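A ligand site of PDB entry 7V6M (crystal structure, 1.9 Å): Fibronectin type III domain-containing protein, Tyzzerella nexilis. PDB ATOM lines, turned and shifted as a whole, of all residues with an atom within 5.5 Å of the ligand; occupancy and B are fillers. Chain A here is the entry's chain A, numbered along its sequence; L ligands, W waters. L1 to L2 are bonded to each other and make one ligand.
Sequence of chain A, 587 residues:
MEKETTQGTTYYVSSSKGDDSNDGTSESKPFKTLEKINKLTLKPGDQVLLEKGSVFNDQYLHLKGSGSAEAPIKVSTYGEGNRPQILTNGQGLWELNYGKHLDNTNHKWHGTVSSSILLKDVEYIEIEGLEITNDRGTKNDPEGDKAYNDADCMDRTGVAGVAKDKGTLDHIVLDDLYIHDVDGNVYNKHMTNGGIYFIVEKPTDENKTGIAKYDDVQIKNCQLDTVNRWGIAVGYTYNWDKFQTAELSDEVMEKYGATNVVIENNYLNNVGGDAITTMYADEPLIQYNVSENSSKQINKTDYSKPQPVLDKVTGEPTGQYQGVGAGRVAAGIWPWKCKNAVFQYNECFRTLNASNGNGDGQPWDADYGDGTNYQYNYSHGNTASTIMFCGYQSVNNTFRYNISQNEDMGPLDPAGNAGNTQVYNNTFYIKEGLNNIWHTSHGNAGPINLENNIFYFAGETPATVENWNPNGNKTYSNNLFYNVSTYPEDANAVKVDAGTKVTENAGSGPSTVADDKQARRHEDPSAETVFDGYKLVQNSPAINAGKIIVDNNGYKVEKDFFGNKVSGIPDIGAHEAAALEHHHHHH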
ATOM      1  N   ASP A 103      17.563 -36.776 -22.861  1.00  0.00           N
ATOM      2  CA  ASP A 103      18.763 -37.593 -22.505  1.00  0.00           C
ATOM      3  C   ASP A 103      18.911 -37.704 -20.977  1.00  0.00           C
ATOM      4  O   ASP A 103      19.410 -38.721 -20.486  1.00  0.00           O
ATOM      5  CB  ASP A 103      20.041 -37.042 -23.145  1.00  0.00           C
ATOM      6  CG  ASP A 103      20.616 -35.818 -22.442  1.00  0.00           C
ATOM      7  OD1 ASP A 103      20.122 -34.708 -22.722  1.00  0.00           O
ATOM      8  OD2 ASP A 103      21.606 -35.970 -21.669  1.00  0.00           O
ATOM      9  N   ASN A 104      18.536 -36.652 -20.255  1.00  0.00           N
ATOM     10  CA  ASN A 104      18.428 -36.644 -18.782  1.00  0.00           C
ATOM     11  C   ASN A 104      16.934 -36.561 -18.438  1.00  0.00           C
ATOM     12  O   ASN A 104      16.297 -35.609 -18.906  1.00  0.00           O
ATOM     13  CB  ASN A 104      19.206 -35.456 -18.219  1.00  0.00           C
ATOM     14  CG  ASN A 104      19.232 -35.406 -16.704  1.00  0.00           C
ATOM     15  OD1 ASN A 104      18.292 -35.804 -16.026  1.00  0.00           O
ATOM     16  ND2 ASN A 104      20.316 -34.868 -16.178  1.00  0.00           N
ATOM     17  N   HIS A 107      15.429 -33.046 -17.425  1.00  0.00           N
ATOM     18  CA  HIS A 107      15.193 -31.898 -18.335  1.00  0.00           C
ATOM     19  C   HIS A 107      13.677 -31.788 -18.602  1.00  0.00           C
ATOM     20  O   HIS A 107      13.050 -32.729 -19.149  1.00  0.00           O
ATOM     21  CB  HIS A 107      15.944 -32.012 -19.679  1.00  0.00           C
ATOM     22  CG  HIS A 107      17.442 -32.042 -19.639  1.00  0.00           C
ATOM     23  ND1 HIS A 107      18.208 -31.233 -18.815  1.00  0.00           N
ATOM     24  CD2 HIS A 107      18.323 -32.754 -20.394  1.00  0.00           C
ATOM     25  CE1 HIS A 107      19.488 -31.473 -19.041  1.00  0.00           C
ATOM     26  NE2 HIS A 107      19.587 -32.413 -20.010  1.00  0.00           N
ATOM     27  N   LYS A 189      17.236 -26.242 -19.779  1.00  0.00           N
ATOM     28  CA  LYS A 189      18.226 -26.324 -20.886  1.00  0.00           C
ATOM     29  C   LYS A 189      17.550 -26.586 -22.234  1.00  0.00           C
ATOM     30  O   LYS A 189      18.160 -26.192 -23.253  1.00  0.00           O
ATOM     31  CB  LYS A 189      19.280 -27.407 -20.571  1.00  0.00           C
ATOM     32  CG  LYS A 189      20.264 -26.961 -19.496  1.00  0.00           C
ATOM     33  CD  LYS A 189      21.430 -27.910 -19.247  1.00  0.00           C
ATOM     34  CE  LYS A 189      22.481 -27.808 -20.318  1.00  0.00           C
ATOM     35  NZ  LYS A 189      23.492 -28.884 -20.230  1.00  0.00           N
ATOM     36  N   HIS A 190      16.398 -27.280 -22.279  1.00  0.00           N
ATOM     37  CA  HIS A 190      15.900 -27.865 -23.562  1.00  0.00           C
ATOM     38  C   HIS A 190      14.437 -27.560 -23.893  1.00  0.00           C
ATOM     39  O   HIS A 190      13.985 -27.907 -25.013  1.00  0.00           O
ATOM     40  CB  HIS A 190      16.289 -29.359 -23.653  1.00  0.00           C
ATOM     41  CG  HIS A 190      17.762 -29.580 -23.555  1.00  0.00           C
ATOM     42  ND1 HIS A 190      18.640 -29.024 -24.479  1.00  0.00           N
ATOM     43  CD2 HIS A 190      18.517 -30.183 -22.620  1.00  0.00           C
ATOM     44  CE1 HIS A 190      19.883 -29.300 -24.099  1.00  0.00           C
ATOM     45  NE2 HIS A 190      19.835 -30.037 -22.982  1.00  0.00           N
ATOM     46  N   TRP A 230      19.354 -19.814 -22.996  1.00  0.00           N
ATOM     47  CA  TRP A 230      20.294 -20.016 -24.140  1.00  0.00           C
ATOM     48  C   TRP A 230      20.374 -18.745 -24.989  1.00  0.00           C
ATOM     49  O   TRP A 230      19.388 -17.956 -25.026  1.00  0.00           O
ATOM     50  CB  TRP A 230      19.887 -21.228 -24.999  1.00  0.00           C
ATOM     51  CG  TRP A 230      21.059 -22.111 -25.311  1.00  0.00           C
ATOM     52  CD1 TRP A 230      22.046 -21.887 -26.226  1.00  0.00           C
ATOM     53  CD2 TRP A 230      21.392 -23.355 -24.660  1.00  0.00           C
ATOM     54  NE1 TRP A 230      22.963 -22.908 -26.194  1.00  0.00           N
ATOM     55  CE2 TRP A 230      22.559 -23.848 -25.265  1.00  0.00           C
ATOM     56  CE3 TRP A 230      20.738 -24.141 -23.699  1.00  0.00           C
ATOM     57  CZ2 TRP A 230      23.147 -25.052 -24.859  1.00  0.00           C
ATOM     58  CZ3 TRP A 230      21.319 -25.337 -23.321  1.00  0.00           C
ATOM     59  CH2 TRP A 230      22.513 -25.782 -23.872  1.00  0.00           C
ATOM     60  N   TYR A 236      18.034 -29.681 -30.682  1.00  0.00           N
ATOM     61  CA  TYR A 236      17.675 -30.725 -29.681  1.00  0.00           C
ATOM     62  C   TYR A 236      16.445 -31.483 -30.159  1.00  0.00           C
ATOM     63  O   TYR A 236      15.452 -30.848 -30.526  1.00  0.00           O
ATOM     64  CB  TYR A 236      17.517 -30.227 -28.247  1.00  0.00           C
ATOM     65  CG  TYR A 236      17.751 -31.361 -27.272  1.00  0.00           C
ATOM     66  CD1 TYR A 236      16.799 -32.360 -27.109  1.00  0.00           C
ATOM     67  CD2 TYR A 236      18.957 -31.492 -26.600  1.00  0.00           C
ATOM     68  CE1 TYR A 236      17.030 -33.452 -26.292  1.00  0.00           C
ATOM     69  CE2 TYR A 236      19.186 -32.572 -25.747  1.00  0.00           C
ATOM     70  CZ  TYR A 236      18.222 -33.552 -25.593  1.00  0.00           C
ATOM     71  OH  TYR A 236      18.408 -34.609 -24.754  1.00  0.00           O
ATOM     72  N   ASP A 274      24.520 -20.550 -22.046  1.00  0.00           N
ATOM     73  CA  ASP A 274      25.440 -20.865 -23.157  1.00  0.00           C
ATOM     74  C   ASP A 274      25.183 -19.904 -24.318  1.00  0.00           C
ATOM     75  O   ASP A 274      23.987 -19.620 -24.642  1.00  0.00           O
ATOM     76  CB  ASP A 274      25.292 -22.315 -23.631  1.00  0.00           C
ATOM     77  CG  ASP A 274      25.727 -23.325 -22.592  1.00  0.00           C
ATOM     78  OD1 ASP A 274      24.863 -23.705 -21.789  1.00  0.00           O
ATOM     79  OD2 ASP A 274      26.923 -23.704 -22.594  1.00  0.00           O
ATOM     80  N   MET A 279      23.267 -28.784 -31.829  1.00  0.00           N
ATOM     81  CA  MET A 279      22.841 -30.032 -31.140  1.00  0.00           C
ATOM     82  C   MET A 279      22.360 -31.011 -32.211  1.00  0.00           C
ATOM     83  O   MET A 279      21.480 -30.637 -33.001  1.00  0.00           O
ATOM     84  CB  MET A 279      21.697 -29.731 -30.157  1.00  0.00           C
ATOM     85  CG  MET A 279      22.049 -28.717 -29.081  1.00  0.00           C
ATOM     86  SD  MET A 279      20.644 -28.168 -28.092  1.00  0.00           S
ATOM     87  CE  MET A 279      21.520 -27.151 -26.896  1.00  0.00           C
ATOM     88  N   TYR A 280      22.897 -32.236 -32.214  1.00  0.00           N
ATOM     89  CA  TYR A 280      22.436 -33.309 -33.124  1.00  0.00           C
ATOM     90  C   TYR A 280      22.491 -32.815 -34.570  1.00  0.00           C
ATOM     91  O   TYR A 280      21.511 -32.992 -35.318  1.00  0.00           O
ATOM     92  CB  TYR A 280      21.050 -33.772 -32.684  1.00  0.00           C
ATOM     93  CG  TYR A 280      21.044 -34.296 -31.267  1.00  0.00           C
ATOM     94  CD1 TYR A 280      21.695 -35.480 -30.958  1.00  0.00           C
ATOM     95  CD2 TYR A 280      20.438 -33.601 -30.241  1.00  0.00           C
ATOM     96  CE1 TYR A 280      21.715 -35.954 -29.659  1.00  0.00           C
ATOM     97  CE2 TYR A 280      20.471 -34.058 -28.933  1.00  0.00           C
ATOM     98  CZ  TYR A 280      21.132 -35.239 -28.644  1.00  0.00           C
ATOM     99  OH  TYR A 280      21.221 -35.667 -27.360  1.00  0.00           O
ATOM    100  N   VAL A 329      26.255 -24.837 -15.233  1.00  0.00           N
ATOM    101  CA  VAL A 329      27.458 -24.931 -16.109  1.00  0.00           C
ATOM    102  C   VAL A 329      27.099 -24.280 -17.438  1.00  0.00           C
ATOM    103  O   VAL A 329      25.967 -24.500 -17.940  1.00  0.00           O
ATOM    104  CB  VAL A 329      27.889 -26.406 -16.327  1.00  0.00           C
ATOM    105  CG1 VAL A 329      28.501 -26.971 -15.053  1.00  0.00           C
ATOM    106  CG2 VAL A 329      26.734 -27.262 -16.792  1.00  0.00           C
ATOM    107  N   ALA A 330      28.021 -23.540 -18.040  1.00  0.00           N
ATOM    108  CA  ALA A 330      27.841 -23.024 -19.410  1.00  0.00           C
ATOM    109  C   ALA A 330      29.207 -22.734 -20.018  1.00  0.00           C
ATOM    110  O   ALA A 330      30.145 -22.335 -19.283  1.00  0.00           O
ATOM    111  CB  ALA A 330      26.959 -21.801 -19.413  1.00  0.00           C
ATOM    112  N   ALA A 331      29.316 -22.943 -21.321  1.00  0.00           N
ATOM    113  CA  ALA A 331      30.494 -22.580 -22.141  1.00  0.00           C
ATOM    114  C   ALA A 331      30.056 -21.574 -23.226  1.00  0.00           C
ATOM    115  O   ALA A 331      28.904 -21.170 -23.276  1.00  0.00           O
ATOM    116  CB  ALA A 331      31.143 -23.840 -22.690  1.00  0.00           C
ATOM    117  N   TRP A 334      29.862 -23.790 -28.993  1.00  0.00           N
ATOM    118  CA  TRP A 334      30.263 -25.219 -28.885  1.00  0.00           C
ATOM    119  C   TRP A 334      29.209 -26.174 -29.421  1.00  0.00           C
ATOM    120  O   TRP A 334      28.059 -25.768 -29.624  1.00  0.00           O
ATOM    121  CB  TRP A 334      30.597 -25.553 -27.429  1.00  0.00           C
ATOM    122  CG  TRP A 334      29.482 -25.385 -26.436  1.00  0.00           C
ATOM    123  CD1 TRP A 334      29.028 -24.245 -25.849  1.00  0.00           C
ATOM    124  CD2 TRP A 334      28.663 -26.454 -25.913  1.00  0.00           C
ATOM    125  NE1 TRP A 334      27.981 -24.541 -24.986  1.00  0.00           N
ATOM    126  CE2 TRP A 334      27.730 -25.886 -25.028  1.00  0.00           C
ATOM    127  CE3 TRP A 334      28.603 -27.830 -26.169  1.00  0.00           C
ATOM    128  CZ2 TRP A 334      26.776 -26.645 -24.349  1.00  0.00           C
ATOM    129  CZ3 TRP A 334      27.688 -28.593 -25.451  1.00  0.00           C
ATOM    130  CH2 TRP A 334      26.783 -28.000 -24.584  1.00  0.00           C
ATOM    131  N   TRP A 336      27.157 -30.100 -29.258  1.00  0.00           N
ATOM    132  CA  TRP A 336      26.598 -31.261 -28.515  1.00  0.00           C
ATOM    133  C   TRP A 336      26.157 -32.306 -29.548  1.00  0.00           C
ATOM    134  O   TRP A 336      25.248 -31.997 -30.350  1.00  0.00           O
ATOM    135  CB  TRP A 336      25.408 -30.830 -27.657  1.00  0.00           C
ATOM    136  CG  TRP A 336      24.745 -32.029 -27.046  1.00  0.00           C
ATOM    137  CD1 TRP A 336      23.565 -32.602 -27.438  1.00  0.00           C
ATOM    138  CD2 TRP A 336      25.265 -32.850 -25.995  1.00  0.00           C
ATOM    139  NE1 TRP A 336      23.290 -33.696 -26.657  1.00  0.00           N
ATOM    140  CE2 TRP A 336      24.309 -33.881 -25.773  1.00  0.00           C
ATOM    141  CE3 TRP A 336      26.397 -32.794 -25.169  1.00  0.00           C
ATOM    142  CZ2 TRP A 336      24.479 -34.843 -24.776  1.00  0.00           C
ATOM    143  CZ3 TRP A 336      26.560 -33.756 -24.207  1.00  0.00           C
ATOM    144  CH2 TRP A 336      25.611 -34.761 -24.003  1.00  0.00           C
ATOM    145  N   ASN A 358      29.879 -21.379 -11.731  1.00  0.00           N
ATOM    146  CA  ASN A 358      29.900 -21.968 -13.088  1.00  0.00           C
ATOM    147  C   ASN A 358      30.919 -23.107 -13.067  1.00  0.00           C
ATOM    148  O   ASN A 358      32.126 -22.844 -12.895  1.00  0.00           O
ATOM    149  CB  ASN A 358      30.261 -20.950 -14.190  1.00  0.00           C
ATOM    150  CG  ASN A 358      30.053 -21.499 -15.597  1.00  0.00           C
ATOM    151  OD1 ASN A 358      29.899 -22.726 -15.784  1.00  0.00           O
ATOM    152  ND2 ASN A 358      30.068 -20.602 -16.593  1.00  0.00           N
ATOM    153  N   ASP A 360      31.899 -24.762 -15.495  1.00  0.00           N
ATOM    154  CA  ASP A 360      32.595 -24.683 -16.796  1.00  0.00           C
ATOM    155  C   ASP A 360      33.125 -23.254 -16.993  1.00  0.00           C
ATOM    156  O   ASP A 360      33.957 -22.845 -16.169  1.00  0.00           O
ATOM    157  CB  ASP A 360      31.681 -25.222 -17.916  1.00  0.00           C
ATOM    158  CG  ASP A 360      31.674 -26.744 -17.924  1.00  0.00           C
ATOM    159  OD1 ASP A 360      32.747 -27.323 -17.788  1.00  0.00           O
ATOM    160  OD2 ASP A 360      30.564 -27.325 -18.073  1.00  0.00           O
ATOM    161  N   GLN A 362      34.467 -22.163 -20.168  1.00  0.00           N
ATOM    162  CA  GLN A 362      35.383 -22.154 -21.347  1.00  0.00           C
ATOM    163  C   GLN A 362      34.726 -21.409 -22.509  1.00  0.00           C
ATOM    164  O   GLN A 362      33.512 -21.515 -22.744  1.00  0.00           O
ATOM    165  CB  GLN A 362      35.745 -23.573 -21.774  1.00  0.00           C
ATOM    166  CG  GLN A 362      36.185 -24.475 -20.611  1.00  0.00           C
ATOM    167  CD  GLN A 362      35.044 -25.222 -19.944  1.00  0.00           C
ATOM    168  OE1 GLN A 362      33.877 -24.928 -20.198  1.00  0.00           O
ATOM    169  NE2 GLN A 362      35.373 -26.158 -19.071  1.00  0.00           N
ATOM    170  N   ASP A 365      34.188 -25.650 -26.233  1.00  0.00           N
ATOM    171  CA  ASP A 365      33.925 -26.946 -25.532  1.00  0.00           C
ATOM    172  C   ASP A 365      33.595 -28.021 -26.578  1.00  0.00           C
ATOM    173  O   ASP A 365      32.451 -28.103 -26.946  1.00  0.00           O
ATOM    174  CB  ASP A 365      32.760 -26.789 -24.540  1.00  0.00           C
ATOM    175  CG  ASP A 365      32.180 -28.102 -23.995  1.00  0.00           C
ATOM    176  OD1 ASP A 365      32.786 -29.186 -24.189  1.00  0.00           O
ATOM    177  OD2 ASP A 365      31.063 -28.032 -23.475  1.00  0.00           O
ATOM    178  N   ASP A 367      32.313 -31.018 -26.817  1.00  0.00           N
ATOM    179  CA  ASP A 367      31.568 -31.842 -25.835  1.00  0.00           C
ATOM    180  C   ASP A 367      31.360 -33.242 -26.443  1.00  0.00           C
ATOM    181  O   ASP A 367      32.060 -33.558 -27.428  1.00  0.00           O
ATOM    182  CB  ASP A 367      30.308 -31.083 -25.403  1.00  0.00           C
ATOM    183  CG  ASP A 367      29.843 -31.381 -23.996  1.00  0.00           C
ATOM    184  OD1 ASP A 367      29.608 -32.570 -23.727  1.00  0.00           O
ATOM    185  OD2 ASP A 367      29.729 -30.401 -23.165  1.00  0.00           O
ATOM    186  N   TYR A 368      30.493 -34.083 -25.890  1.00  0.00           N
ATOM    187  CA  TYR A 368      30.154 -35.380 -26.533  1.00  0.00           C
ATOM    188  C   TYR A 368      29.918 -35.102 -28.017  1.00  0.00           C
ATOM    189  O   TYR A 368      29.216 -34.127 -28.328  1.00  0.00           O
ATOM    190  CB  TYR A 368      28.906 -35.991 -25.930  1.00  0.00           C
ATOM    191  CG  TYR A 368      29.066 -36.663 -24.586  1.00  0.00           C
ATOM    192  CD1 TYR A 368      30.240 -36.569 -23.846  1.00  0.00           C
ATOM    193  CD2 TYR A 368      28.013 -37.401 -24.050  1.00  0.00           C
ATOM    194  CE1 TYR A 368      30.367 -37.191 -22.619  1.00  0.00           C
ATOM    195  CE2 TYR A 368      28.118 -38.014 -22.818  1.00  0.00           C
ATOM    196  CZ  TYR A 368      29.306 -37.930 -22.116  1.00  0.00           C
ATOM    197  OH  TYR A 368      29.360 -38.500 -20.890  1.00  0.00           O
ATOM    198  N   MET A 388      37.838 -27.122 -23.461  1.00  0.00           N
ATOM    199  CA  MET A 388      37.488 -28.411 -22.819  1.00  0.00           C
ATOM    200  C   MET A 388      37.211 -29.456 -23.906  1.00  0.00           C
ATOM    201  O   MET A 388      36.534 -29.133 -24.901  1.00  0.00           O
ATOM    202  CB  MET A 388      36.279 -28.279 -21.876  1.00  0.00           C
ATOM    203  CG  MET A 388      35.853 -29.626 -21.288  1.00  0.00           C
ATOM    204  SD  MET A 388      34.703 -29.468 -19.926  1.00  0.00           S
ATOM    205  CE  MET A 388      33.272 -28.741 -20.728  1.00  0.00           C
ATOM    206  N   CYS A 390      35.199 -32.768 -23.482  1.00  0.00           N
ATOM    207  CA  CYS A 390      34.332 -33.182 -22.347  1.00  0.00           C
ATOM    208  C   CYS A 390      33.919 -34.663 -22.419  1.00  0.00           C
ATOM    209  O   CYS A 390      32.912 -34.978 -23.114  1.00  0.00           O
ATOM    210  CB  CYS A 390      33.104 -32.305 -22.193  1.00  0.00           C
ATOM    211  SG  CYS A 390      32.262 -32.555 -20.607  1.00  0.00           S
HETATM  212  C1  LIG L   1      29.710 -30.011 -20.308  1.00  0.00           C
HETATM  213  C2  LIG L   1      28.435 -30.896 -20.310  1.00  0.00           C
HETATM  214  C3  LIG L   1      27.213 -30.256 -20.981  1.00  0.00           C
HETATM  215  C4  LIG L   1      27.149 -28.754 -20.708  1.00  0.00           C
HETATM  216  C5  LIG L   1      28.447 -28.107 -21.192  1.00  0.00           C
HETATM  217  C6  LIG L   1      28.361 -26.590 -21.039  1.00  0.00           C
HETATM  218  C7  LIG L   1      28.682 -33.326 -20.138  1.00  0.00           C
HETATM  219  C8  LIG L   1      29.004 -34.597 -20.815  1.00  0.00           C
HETATM  220  N1  LIG L   1      28.737 -32.195 -20.864  1.00  0.00           N
HETATM  221  O1  LIG L   1      30.380 -30.143 -19.050  1.00  0.00           O
HETATM  222  O2  LIG L   1      26.039 -30.844 -20.393  1.00  0.00           O
HETATM  223  O3  LIG L   1      25.982 -28.164 -21.262  1.00  0.00           O
HETATM  224  O4  LIG L   1      29.544 -28.596 -20.386  1.00  0.00           O
HETATM  225  O5  LIG L   1      28.619 -26.180 -19.698  1.00  0.00           O
HETATM  226  O6  LIG L   1      28.354 -33.316 -18.965  1.00  0.00           O
HETATM  227  C1  LG2 L   2      25.262 -31.610 -21.309  1.00  0.00           C
HETATM  228  C2  LG2 L   2      24.237 -32.438 -20.502  1.00  0.00           C
HETATM  229  C3  LG2 L   2      23.156 -33.052 -21.396  1.00  0.00           C
HETATM  230  C4  LG2 L   2      22.571 -31.981 -22.312  1.00  0.00           C
HETATM  231  C5  LG2 L   2      23.713 -31.328 -23.104  1.00  0.00           C
HETATM  232  C6  LG2 L   2      23.272 -30.249 -24.052  1.00  0.00           C
HETATM  233  O1  LG2 L   2      24.916 -33.485 -19.873  1.00  0.00           O
HETATM  234  O2  LG2 L   2      22.125 -33.673 -20.616  1.00  0.00           O
HETATM  235  O3  LG2 L   2      21.906 -31.023 -21.508  1.00  0.00           O
HETATM  236  O4  LG2 L   2      24.623 -30.716 -22.220  1.00  0.00           O
HETATM  237  O5  LG2 L   2      22.462 -30.733 -25.130  1.00  0.00           O
HETATM  238  O   HOH W   1      22.372 -33.625 -17.772  1.00  0.00           O
HETATM  239  O   HOH W   2      25.296 -25.876 -20.137  1.00  0.00           O
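The side-chain carboxylate (OD2) of Asp 365 lies close to an oxygen (O4) of LIG L1, at 3.5 Å. Residues that only touch the ligand: Val 329, Trp 334, Tyr 368, Asp 274, Met 388, Ala 331 and Tyr 236. Hydrophobic or aromatic side chains within 4 Å of the ligand: His 107, His 190, Tyr 236, Val 329, Trp 334, Trp 336, Tyr 368 and Met 388. Of the 23 residues printed, 17 come within 4 Å of the ligand. The nearest printed residue that does not touch the ligand is Met 279 (4.1 Å).
The side-chain carboxylate (OD1) of Asp 103 lies within hydrogen-bond range of the side-chain hydroxyl (OH) of Tyr 236. NE2 of Gln 362 lies within hydrogen-bond range of OD1 of Asp 360 (3.1 Å). The backbone NH (N) of Asp 367 sits at hydrogen-bond distance from the side-chain carboxylate (OD1) of Asp 365. The side-chain hydroxyl (OH) of Tyr 280 is in hydrogen-bond range of the indole nitrogen (NE1) of Trp 336 (2.9 Å). The backbone NH of Ala 330 lies within hydrogen-bond range of the side-chain amide oxygen of Asn 358. The side-chain carboxylate (OD2) of Asp 274 is in hydrogen-bond range of the indole nitrogen (NE1) of Trp 334, 2.7 Å away. OD2 of Asp 274 lies within hydrogen-bond range of N of Ala 331 (2.8 Å). The side-chain amide nitrogen (NE2) of Gln 362 lies within hydrogen-bond range of the side-chain sulfur (SD) of Met 388 (3.5 Å).
Water W2 lies within hydrogen-bond range of O3 of LIG L1 (2.6 Å), O of Val 329 (2.7 Å) and OD1 of Asp 274 (2.8 Å). Water W1 bridges O2 of LG2 L2 and ND2 of Asn 104.
OD2 of Asp 103 is in hydrogen-bond range of O2 of LG2 L2 (2.6 Å). O3 of LG2 L2 lies within hydrogen-bond range of NE2 of His 190 (2.7 Å). The side-chain carboxylate of Asp 360 sits at hydrogen-bond distance from an oxygen (O5) of LIG L1, 2.8 Å away. The side-chain amino group (NZ) of Lys 189 sits at hydrogen-bond distance from an oxygen (O3) of LIG L1, 2.8 Å away. A nitrogen (N1) of LIG L1 is in hydrogen-bond range of the side-chain carboxylate (OD1) of Asp 367 (3.0 Å). A ring nitrogen (NE2) of His 107 is in hydrogen-bond range of an oxygen (O2) of LG2 L2 (2.9 Å). NE1 of Trp 336 sits close to O5 of LG2 L2, 3.4 Å away. O5 of LIG L1 sits at hydrogen-bond distance from N of Ala 330 (3.2 Å). SG of Cys 390 is in hydrogen-bond range of O1 of LIG L1.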
